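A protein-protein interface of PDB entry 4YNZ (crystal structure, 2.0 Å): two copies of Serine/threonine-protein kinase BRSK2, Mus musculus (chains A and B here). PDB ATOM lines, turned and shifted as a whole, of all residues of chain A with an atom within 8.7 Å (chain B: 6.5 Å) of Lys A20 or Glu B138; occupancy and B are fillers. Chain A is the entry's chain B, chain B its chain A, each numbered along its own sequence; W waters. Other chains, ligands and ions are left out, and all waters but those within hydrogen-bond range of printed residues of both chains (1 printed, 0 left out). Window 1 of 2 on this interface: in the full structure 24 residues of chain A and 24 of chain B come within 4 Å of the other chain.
Along chain B the printed residues that touch a printed residue of chain A span positions 20 to 138. Along chain A the printed residues that touch a printed residue of chain B span positions 1 to 138. Among the printed residues, Asp or Glu carboxylates within 4 Å of a Lys or Arg side-chain nitrogen of the other chain: Lys A20 with Glu B95 (2.6 Å), Lys A20 with Glu B138 (3.4 Å) and Glu A138 with Lys B20 (3.6 Å).
The side-chain carboxylate (OE2) of Glu B138 lies within salt-bridge range of the side-chain amino group (NZ) of Lys A20, 3.4 Å away. The side-chain amino group (NZ) of Lys A20 lies within salt-bridge range of the side-chain carboxylate (OE1) of Glu B95 (2.6 Å). The side-chain amino group (NZ) of Lys B20 lies within salt-bridge range of the side-chain carboxylate (OE2) of Glu A138 (3.6 Å).
Lys A20 touches Glu B138, and with the chains exchanged Glu A138 touches Lys B20. 2 positions are printed for both chains. Of the 4 pairs that touch across the chains among the printed residues, 2 have their exchanged pair printed and touching as well.
Water W1 lies within hydrogen-bond range of the backbone NH (N) of Gly A1 (2.6 Å), the side-chain hydroxyl (OG1) of Thr A17 (2.9 Å) and the side-chain carboxylate (OE2) of Glu B95 (3.0 Å).
Among the printed residues, pairs that only touch across the chains: Gly A1 with Phe B97.
Printed residues of chain B within 4 Å of Gly A1: Phe B97. Of chain B, only Glu B95 and Glu B138 come within 4 Å of Lys A20. Of the printed residues of chain A, Glu B95 touches Lys A20. Of the printed residues of chain A, Phe B97 touches Gly A1. No residue of chain A comes within 4 Å of Pro B137. Glu B138 touches one residue of chain A. The nearest printed residue of chain A that does not touch Glu B138 is Leu A25 (7.0 Å). The nearest printed residue of chain A that does not touch Lys B20 is Lys A20 (4.7 Å).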
ATOM      1  N   GLY A   1     -21.331 -16.734 -23.452  1.00  0.00           N
ATOM      2  CA  GLY A   1     -20.818 -16.020 -22.302  1.00  0.00           C
ATOM      3  C   GLY A   1     -21.808 -14.987 -21.832  1.00  0.00           C
ATOM      4  O   GLY A   1     -22.831 -14.764 -22.484  1.00  0.00           O
ATOM      5  N   PRO A   2     -21.512 -14.339 -20.692  1.00  0.00           N
ATOM      6  CA  PRO A   2     -22.450 -13.325 -20.197  1.00  0.00           C
ATOM      7  C   PRO A   2     -22.570 -12.162 -21.174  1.00  0.00           C
ATOM      8  O   PRO A   2     -21.645 -11.897 -21.948  1.00  0.00           O
ATOM      9  CB  PRO A   2     -21.818 -12.865 -18.868  1.00  0.00           C
ATOM     10  CG  PRO A   2     -20.374 -13.230 -18.977  1.00  0.00           C
ATOM     11  CD  PRO A   2     -20.315 -14.454 -19.836  1.00  0.00           C
ATOM     12  N   LYS A  16     -16.865 -21.447 -27.061  1.00  0.00           N
ATOM     13  CA  LYS A  16     -18.018 -21.965 -26.326  1.00  0.00           C
ATOM     14  C   LYS A  16     -17.879 -21.929 -24.807  1.00  0.00           C
ATOM     15  O   LYS A  16     -16.772 -21.964 -24.252  1.00  0.00           O
ATOM     16  CB  LYS A  16     -18.361 -23.375 -26.804  1.00  0.00           C
ATOM     17  CG  LYS A  16     -17.285 -24.402 -26.540  1.00  0.00           C
ATOM     18  CD  LYS A  16     -17.611 -25.719 -27.240  1.00  0.00           C
ATOM     19  CE  LYS A  16     -17.542 -26.899 -26.264  1.00  0.00           C
ATOM     20  NZ  LYS A  16     -17.479 -28.214 -26.972  1.00  0.00           N
ATOM     21  N   THR A  17     -19.017 -21.876 -24.123  1.00  0.00           N
ATOM     22  CA  THR A  17     -19.012 -21.967 -22.675  1.00  0.00           C
ATOM     23  C   THR A  17     -18.634 -23.397 -22.274  1.00  0.00           C
ATOM     24  O   THR A  17     -19.158 -24.354 -22.833  1.00  0.00           O
ATOM     25  CB  THR A  17     -20.407 -21.594 -22.101  1.00  0.00           C
ATOM     26  OG1 THR A  17     -20.658 -20.206 -22.343  1.00  0.00           O
ATOM     27  CG2 THR A  17     -20.459 -21.861 -20.611  1.00  0.00           C
ATOM     28  N   LEU A  18     -17.709 -23.549 -21.329  1.00  0.00           N
ATOM     29  CA  LEU A  18     -17.341 -24.888 -20.873  1.00  0.00           C
ATOM     30  C   LEU A  18     -18.150 -25.295 -19.647  1.00  0.00           C
ATOM     31  O   LEU A  18     -18.495 -26.461 -19.490  1.00  0.00           O
ATOM     32  CB  LEU A  18     -15.837 -25.002 -20.594  1.00  0.00           C
ATOM     33  CG  LEU A  18     -14.959 -24.917 -21.854  1.00  0.00           C
ATOM     34  CD1 LEU A  18     -13.481 -25.002 -21.535  1.00  0.00           C
ATOM     35  CD2 LEU A  18     -15.366 -26.003 -22.836  1.00  0.00           C
ATOM     36  N   GLY A  19     -18.456 -24.331 -18.785  1.00  0.00           N
ATOM     37  CA  GLY A  19     -19.146 -24.631 -17.544  1.00  0.00           C
ATOM     38  C   GLY A  19     -19.334 -23.392 -16.701  1.00  0.00           C
ATOM     39  O   GLY A  19     -18.774 -22.335 -16.995  1.00  0.00           O
ATOM     40  N   LYS A  20     -20.144 -23.504 -15.658  1.00  0.00           N
ATOM     41  CA  LYS A  20     -20.359 -22.368 -14.780  1.00  0.00           C
ATOM     42  C   LYS A  20     -20.782 -22.799 -13.401  1.00  0.00           C
ATOM     43  O   LYS A  20     -21.065 -23.971 -13.155  1.00  0.00           O
ATOM     44  CB  LYS A  20     -21.405 -21.414 -15.352  1.00  0.00           C
ATOM     45  CG  LYS A  20     -22.822 -21.914 -15.317  1.00  0.00           C
ATOM     46  CD  LYS A  20     -23.633 -21.277 -16.434  1.00  0.00           C
ATOM     47  CE  LYS A  20     -23.373 -21.972 -17.767  1.00  0.00           C
ATOM     48  NZ  LYS A  20     -24.114 -21.320 -18.869  1.00  0.00           N
ATOM     49  N   GLY A  21     -20.826 -21.824 -12.506  1.00  0.00           N
ATOM     50  CA  GLY A  21     -21.220 -22.061 -11.137  1.00  0.00           C
ATOM     51  C   GLY A  21     -21.183 -20.727 -10.439  1.00  0.00           C
ATOM     52  O   GLY A  21     -21.095 -19.683 -11.105  1.00  0.00           O
ATOM     53  N   GLN A  22     -21.232 -20.755  -9.110  1.00  0.00           N
ATOM     54  CA  GLN A  22     -21.334 -19.528  -8.330  1.00  0.00           C
ATOM     55  C   GLN A  22     -20.051 -18.690  -8.370  1.00  0.00           C
ATOM     56  O   GLN A  22     -20.099 -17.473  -8.213  1.00  0.00           O
ATOM     57  CB  GLN A  22     -21.743 -19.842  -6.887  1.00  0.00           C
ATOM     58  CG  GLN A  22     -22.407 -18.675  -6.171  1.00  0.00           C
ATOM     59  CD  GLN A  22     -23.650 -18.164  -6.892  1.00  0.00           C
ATOM     60  OE1 GLN A  22     -23.878 -16.954  -6.984  1.00  0.00           O
ATOM     61  NE2 GLN A  22     -24.462 -19.086  -7.401  1.00  0.00           N
ATOM     62  N   THR A  23     -18.909 -19.339  -8.594  1.00  0.00           N
ATOM     63  CA  THR A  23     -17.627 -18.626  -8.613  1.00  0.00           C
ATOM     64  C   THR A  23     -17.260 -18.082 -10.001  1.00  0.00           C
ATOM     65  O   THR A  23     -16.183 -17.510 -10.186  1.00  0.00           O
ATOM     66  CB  THR A  23     -16.459 -19.489  -8.041  1.00  0.00           C
ATOM     67  OG1 THR A  23     -16.224 -20.627  -8.880  1.00  0.00           O
ATOM     68  CG2 THR A  23     -16.779 -19.964  -6.626  1.00  0.00           C
ATOM     69  N   GLY A  24     -18.155 -18.252 -10.971  1.00  0.00           N
ATOM     70  CA  GLY A  24     -17.935 -17.700 -12.295  1.00  0.00           C
ATOM     71  C   GLY A  24     -18.216 -18.617 -13.479  1.00  0.00           C
ATOM     72  O   GLY A  24     -18.568 -19.789 -13.324  1.00  0.00           O
ATOM     73  N   LEU A  25     -18.051 -18.065 -14.677  1.00  0.00           N
ATOM     74  CA  LEU A  25     -18.364 -18.777 -15.904  1.00  0.00           C
ATOM     75  C   LEU A  25     -17.070 -19.096 -16.648  1.00  0.00           C
ATOM     76  O   LEU A  25     -16.188 -18.238 -16.778  1.00  0.00           O
ATOM     77  CB  LEU A  25     -19.321 -17.929 -16.746  1.00  0.00           C
ATOM     78  CG  LEU A  25     -19.863 -18.373 -18.107  1.00  0.00           C
ATOM     79  CD1 LEU A  25     -18.834 -18.257 -19.212  1.00  0.00           C
ATOM     80  CD2 LEU A  25     -20.336 -19.760 -18.026  1.00  0.00           C
ATOM     81  N   VAL A  26     -16.940 -20.322 -17.137  1.00  0.00           N
ATOM     82  CA  VAL A  26     -15.707 -20.700 -17.827  1.00  0.00           C
ATOM     83  C   VAL A  26     -15.949 -20.938 -19.305  1.00  0.00           C
ATOM     84  O   VAL A  26     -16.817 -21.735 -19.670  1.00  0.00           O
ATOM     85  CB  VAL A  26     -15.047 -21.965 -17.214  1.00  0.00           C
ATOM     86  CG1 VAL A  26     -13.745 -22.274 -17.931  1.00  0.00           C
ATOM     87  CG2 VAL A  26     -14.805 -21.783 -15.731  1.00  0.00           C
ATOM     88  N   LYS A  27     -15.179 -20.247 -20.146  1.00  0.00           N
ATOM     89  CA  LYS A  27     -15.226 -20.425 -21.596  1.00  0.00           C
ATOM     90  C   LYS A  27     -13.878 -20.867 -22.161  1.00  0.00           C
ATOM     91  O   LYS A  27     -12.823 -20.553 -21.612  1.00  0.00           O
ATOM     92  CB  LYS A  27     -15.638 -19.128 -22.295  1.00  0.00           C
ATOM     93  CG  LYS A  27     -17.067 -18.702 -22.011  1.00  0.00           C
ATOM     94  CD  LYS A  27     -17.402 -17.365 -22.651  1.00  0.00           C
ATOM     95  CE  LYS A  27     -18.153 -17.544 -23.953  1.00  0.00           C
ATOM     96  NZ  LYS A  27     -18.524 -16.232 -24.575  1.00  0.00           N
ATOM     97  N   LYS A  41     -11.810 -18.030 -17.157  1.00  0.00           N
ATOM     98  CA  LYS A  41     -12.827 -17.898 -16.126  1.00  0.00           C
ATOM     99  C   LYS A  41     -13.225 -16.447 -15.950  1.00  0.00           C
ATOM    100  O   LYS A  41     -12.382 -15.588 -15.664  1.00  0.00           O
ATOM    101  CB  LYS A  41     -12.365 -18.519 -14.795  1.00  0.00           C
ATOM    102  CG  LYS A  41     -13.410 -18.430 -13.685  1.00  0.00           C
ATOM    103  CD  LYS A  41     -13.333 -19.617 -12.743  1.00  0.00           C
ATOM    104  CE  LYS A  41     -14.570 -19.719 -11.865  1.00  0.00           C
ATOM    105  NZ  LYS A  41     -14.680 -21.079 -11.252  1.00  0.00           N
ATOM    106  N   ILE A  42     -14.516 -16.185 -16.151  1.00  0.00           N
ATOM    107  CA  ILE A  42     -15.081 -14.844 -16.085  1.00  0.00           C
ATOM    108  C   ILE A  42     -15.783 -14.610 -14.748  1.00  0.00           C
ATOM    109  O   ILE A  42     -16.717 -15.339 -14.398  1.00  0.00           O
ATOM    110  CB  ILE A  42     -16.120 -14.661 -17.201  1.00  0.00           C
ATOM    111  CG1 ILE A  42     -15.470 -14.880 -18.569  1.00  0.00           C
ATOM    112  CG2 ILE A  42     -16.798 -13.306 -17.093  1.00  0.00           C
ATOM    113  CD1 ILE A  42     -16.439 -15.031 -19.682  1.00  0.00           C
ATOM    114  N   GLU A 138     -14.833 -32.044  -7.622  1.00  0.00           N
ATOM    115  CA  GLU A 138     -14.854 -31.314  -8.886  1.00  0.00           C
ATOM    116  C   GLU A 138     -13.662 -30.359  -9.111  1.00  0.00           C
ATOM    117  O   GLU A 138     -13.446 -29.878 -10.225  1.00  0.00           O
ATOM    118  CB  GLU A 138     -16.161 -30.544  -9.045  1.00  0.00           C
ATOM    119  CG  GLU A 138     -16.331 -29.414  -8.040  1.00  0.00           C
ATOM    120  CD  GLU A 138     -17.574 -28.598  -8.327  1.00  0.00           C
ATOM    121  OE1 GLU A 138     -18.231 -28.156  -7.363  1.00  0.00           O
ATOM    122  OE2 GLU A 138     -17.896 -28.404  -9.522  1.00  0.00           O
ATOM    123  N   LYS B  20     -22.404 -30.061 -14.345  1.00  0.00           N
ATOM    124  CA  LYS B  20     -23.359 -30.387 -13.294  1.00  0.00           C
ATOM    125  C   LYS B  20     -23.975 -29.133 -12.742  1.00  0.00           C
ATOM    126  O   LYS B  20     -23.472 -28.036 -12.979  1.00  0.00           O
ATOM    127  CB  LYS B  20     -22.690 -31.156 -12.154  1.00  0.00           C
ATOM    128  CG  LYS B  20     -21.908 -30.298 -11.195  1.00  0.00           C
ATOM    129  CD  LYS B  20     -20.447 -30.210 -11.599  1.00  0.00           C
ATOM    130  CE  LYS B  20     -19.661 -31.446 -11.158  1.00  0.00           C
ATOM    131  NZ  LYS B  20     -18.261 -31.334 -11.611  1.00  0.00           N
ATOM    132  N   GLU B  95     -23.619 -22.868 -26.231  1.00  0.00           N
ATOM    133  CA  GLU B  95     -24.944 -22.370 -25.980  1.00  0.00           C
ATOM    134  C   GLU B  95     -25.228 -21.092 -26.770  1.00  0.00           C
ATOM    135  O   GLU B  95     -24.308 -20.425 -27.270  1.00  0.00           O
ATOM    136  CB  GLU B  95     -25.230 -22.251 -24.472  1.00  0.00           C
ATOM    137  CG  GLU B  95     -24.255 -21.397 -23.705  1.00  0.00           C
ATOM    138  CD  GLU B  95     -24.727 -21.092 -22.291  1.00  0.00           C
ATOM    139  OE1 GLU B  95     -24.402 -21.884 -21.381  1.00  0.00           O
ATOM    140  OE2 GLU B  95     -25.407 -20.052 -22.096  1.00  0.00           O
ATOM    141  N   LEU B  96     -26.510 -20.792 -26.932  1.00  0.00           N
ATOM    142  CA  LEU B  96     -26.935 -19.694 -27.814  1.00  0.00           C
ATOM    143  C   LEU B  96     -26.178 -18.396 -27.571  1.00  0.00           C
ATOM    144  O   LEU B  96     -25.724 -17.749 -28.516  1.00  0.00           O
ATOM    145  CB  LEU B  96     -28.435 -19.447 -27.650  1.00  0.00           C
ATOM    146  CG  LEU B  96     -29.047 -18.427 -28.611  1.00  0.00           C
ATOM    147  CD1 LEU B  96     -28.868 -18.870 -30.077  1.00  0.00           C
ATOM    148  CD2 LEU B  96     -30.527 -18.229 -28.289  1.00  0.00           C
ATOM    149  N   PHE B  97     -26.042 -17.999 -26.310  1.00  0.00           N
ATOM    150  CA  PHE B  97     -25.382 -16.726 -26.032  1.00  0.00           C
ATOM    151  C   PHE B  97     -23.869 -16.715 -26.351  1.00  0.00           C
ATOM    152  O   PHE B  97     -23.242 -15.641 -26.371  1.00  0.00           O
ATOM    153  CB  PHE B  97     -25.640 -16.300 -24.577  1.00  0.00           C
ATOM    154  CG  PHE B  97     -26.972 -15.653 -24.361  1.00  0.00           C
ATOM    155  CD1 PHE B  97     -28.000 -15.819 -25.273  1.00  0.00           C
ATOM    156  CD2 PHE B  97     -27.190 -14.842 -23.258  1.00  0.00           C
ATOM    157  CE1 PHE B  97     -29.229 -15.204 -25.076  1.00  0.00           C
ATOM    158  CE2 PHE B  97     -28.421 -14.219 -23.063  1.00  0.00           C
ATOM    159  CZ  PHE B  97     -29.429 -14.401 -23.965  1.00  0.00           C
ATOM    160  N   LYS B 136     -34.057 -20.450 -19.765  1.00  0.00           N
ATOM    161  CA  LYS B 136     -32.961 -19.505 -19.650  1.00  0.00           C
ATOM    162  C   LYS B 136     -31.952 -19.800 -20.763  1.00  0.00           C
ATOM    163  O   LYS B 136     -31.997 -20.871 -21.359  1.00  0.00           O
ATOM    164  CB  LYS B 136     -32.345 -19.565 -18.249  1.00  0.00           C
ATOM    165  CG  LYS B 136     -31.504 -20.783 -17.955  1.00  0.00           C
ATOM    166  CD  LYS B 136     -31.104 -20.822 -16.467  1.00  0.00           C
ATOM    167  CE  LYS B 136     -32.244 -21.274 -15.551  1.00  0.00           C
ATOM    168  NZ  LYS B 136     -32.763 -22.632 -15.915  1.00  0.00           N
ATOM    169  N   PRO B 137     -31.059 -18.846 -21.057  1.00  0.00           N
ATOM    170  CA  PRO B 137     -30.109 -19.022 -22.170  1.00  0.00           C
ATOM    171  C   PRO B 137     -29.306 -20.313 -22.125  1.00  0.00           C
ATOM    172  O   PRO B 137     -29.080 -20.918 -23.174  1.00  0.00           O
ATOM    173  CB  PRO B 137     -29.176 -17.810 -22.029  1.00  0.00           C
ATOM    174  CG  PRO B 137     -30.065 -16.750 -21.420  1.00  0.00           C
ATOM    175  CD  PRO B 137     -30.932 -17.512 -20.428  1.00  0.00           C
ATOM    176  N   GLU B 138     -28.900 -20.750 -20.938  1.00  0.00           N
ATOM    177  CA  GLU B 138     -28.112 -21.973 -20.872  1.00  0.00           C
ATOM    178  C   GLU B 138     -28.909 -23.230 -21.224  1.00  0.00           C
ATOM    179  O   GLU B 138     -28.307 -24.294 -21.404  1.00  0.00           O
ATOM    180  CB  GLU B 138     -27.438 -22.138 -19.510  1.00  0.00           C
ATOM    181  CG  GLU B 138     -28.391 -22.595 -18.405  1.00  0.00           C
ATOM    182  CD  GLU B 138     -27.673 -22.947 -17.116  1.00  0.00           C
ATOM    183  OE1 GLU B 138     -28.347 -23.096 -16.076  1.00  0.00           O
ATOM    184  OE2 GLU B 138     -26.431 -23.071 -17.138  1.00  0.00           O
ATOM    185  N   ASN B 139     -30.244 -23.123 -21.301  1.00  0.00           N
ATOM    186  CA  ASN B 139     -31.080 -24.234 -21.776  1.00  0.00           C
ATOM    187  C   ASN B 139     -31.116 -24.310 -23.304  1.00  0.00           C
ATOM    188  O   ASN B 139     -31.670 -25.249 -23.870  1.00  0.00           O
ATOM    189  CB  ASN B 139     -32.539 -24.100 -21.300  1.00  0.00           C
ATOM    190  CG  ASN B 139     -32.668 -24.124 -19.804  1.00  0.00           C
ATOM    191  OD1 ASN B 139     -33.262 -23.227 -19.207  1.00  0.00           O
ATOM    192  ND2 ASN B 139     -32.068 -25.136 -19.176  1.00  0.00           N
ATOM    193  N   LEU B 140     -30.579 -23.290 -23.964  1.00  0.00           N
ATOM    194  CA  LEU B 140     -30.690 -23.192 -25.412  1.00  0.00           C
ATOM    195  C   LEU B 140     -29.372 -23.649 -26.024  1.00  0.00           C
ATOM    196  O   LEU B 140     -28.463 -22.859 -26.288  1.00  0.00           O
ATOM    197  CB  LEU B 140     -31.081 -21.775 -25.843  1.00  0.00           C
ATOM    198  CG  LEU B 140     -32.356 -21.211 -25.192  1.00  0.00           C
ATOM    199  CD1 LEU B 140     -32.548 -19.756 -25.572  1.00  0.00           C
ATOM    200  CD2 LEU B 140     -33.578 -21.999 -25.594  1.00  0.00           C
ATOM    201  N   LEU B 141     -29.264 -24.953 -26.205  1.00  0.00           N
ATOM    202  CA  LEU B 141     -28.023 -25.528 -26.680  1.00  0.00           C
ATOM    203  C   LEU B 141     -27.897 -25.358 -28.185  1.00  0.00           C
ATOM    204  O   LEU B 141     -28.892 -25.219 -28.887  1.00  0.00           O
ATOM    205  CB  LEU B 141     -27.951 -27.014 -26.315  1.00  0.00           C
ATOM    206  CG  LEU B 141     -28.162 -27.354 -24.837  1.00  0.00           C
ATOM    207  CD1 LEU B 141     -27.842 -28.840 -24.585  1.00  0.00           C
ATOM    208  CD2 LEU B 141     -27.298 -26.444 -23.978  1.00  0.00           C
ATOM    209  N   ALA B 151     -32.983 -27.766 -23.873  1.00  0.00           N
ATOM    210  CA  ALA B 151     -32.707 -28.834 -22.911  1.00  0.00           C
ATOM    211  C   ALA B 151     -33.481 -28.569 -21.604  1.00  0.00           C
ATOM    212  O   ALA B 151     -33.947 -27.443 -21.369  1.00  0.00           O
ATOM    213  CB  ALA B 151     -31.210 -28.903 -22.607  1.00  0.00           C
ATOM    214  N   ASP B 152     -33.588 -29.608 -20.778  1.00  0.00           N
ATOM    215  CA  ASP B 152     -34.101 -29.520 -19.401  1.00  0.00           C
ATOM    216  C   ASP B 152     -35.575 -29.213 -19.227  1.00  0.00           C
ATOM    217  O   ASP B 152     -35.993 -28.655 -18.217  1.00  0.00           O
ATOM    218  CB  ASP B 152     -33.266 -28.551 -18.576  1.00  0.00           C
ATOM    219  CG  ASP B 152     -31.863 -29.090 -18.310  1.00  0.00           C
ATOM    220  OD1 ASP B 152     -31.745 -30.279 -17.943  1.00  0.00           O
ATOM    221  OD2 ASP B 152     -30.888 -28.335 -18.505  1.00  0.00           O
ATOM    222  N   GLN B 159     -35.293 -27.353  -9.123  1.00  0.00           N
ATOM    223  CA  GLN B 159     -34.601 -26.108  -8.775  1.00  0.00           C
ATOM    224  C   GLN B 159     -35.003 -25.633  -7.379  1.00  0.00           C
ATOM    225  O   GLN B 159     -34.320 -24.805  -6.773  1.00  0.00           O
ATOM    226  CB  GLN B 159     -34.877 -25.011  -9.812  1.00  0.00           C
ATOM    227  CG  GLN B 159     -34.357 -25.313 -11.226  1.00  0.00           C
ATOM    228  CD  GLN B 159     -32.902 -24.908 -11.439  1.00  0.00           C
ATOM    229  OE1 GLN B 159     -32.028 -25.199 -10.617  1.00  0.00           O
ATOM    230  NE2 GLN B 159     -32.641 -24.225 -12.544  1.00  0.00           N
ATOM    231  N   SER B 171     -32.629 -18.311 -12.169  1.00  0.00           N
ATOM    232  CA  SER B 171     -32.269 -17.127 -12.955  1.00  0.00           C
ATOM    233  C   SER B 171     -33.447 -16.175 -13.173  1.00  0.00           C
ATOM    234  O   SER B 171     -34.117 -16.209 -14.212  1.00  0.00           O
ATOM    235  CB  SER B 171     -31.632 -17.513 -14.290  1.00  0.00           C
ATOM    236  OG  SER B 171     -30.234 -17.666 -14.175  1.00  0.00           O
HETATM  237  O   HOH W   1     -22.929 -18.424 -22.276  1.00  0.00           O
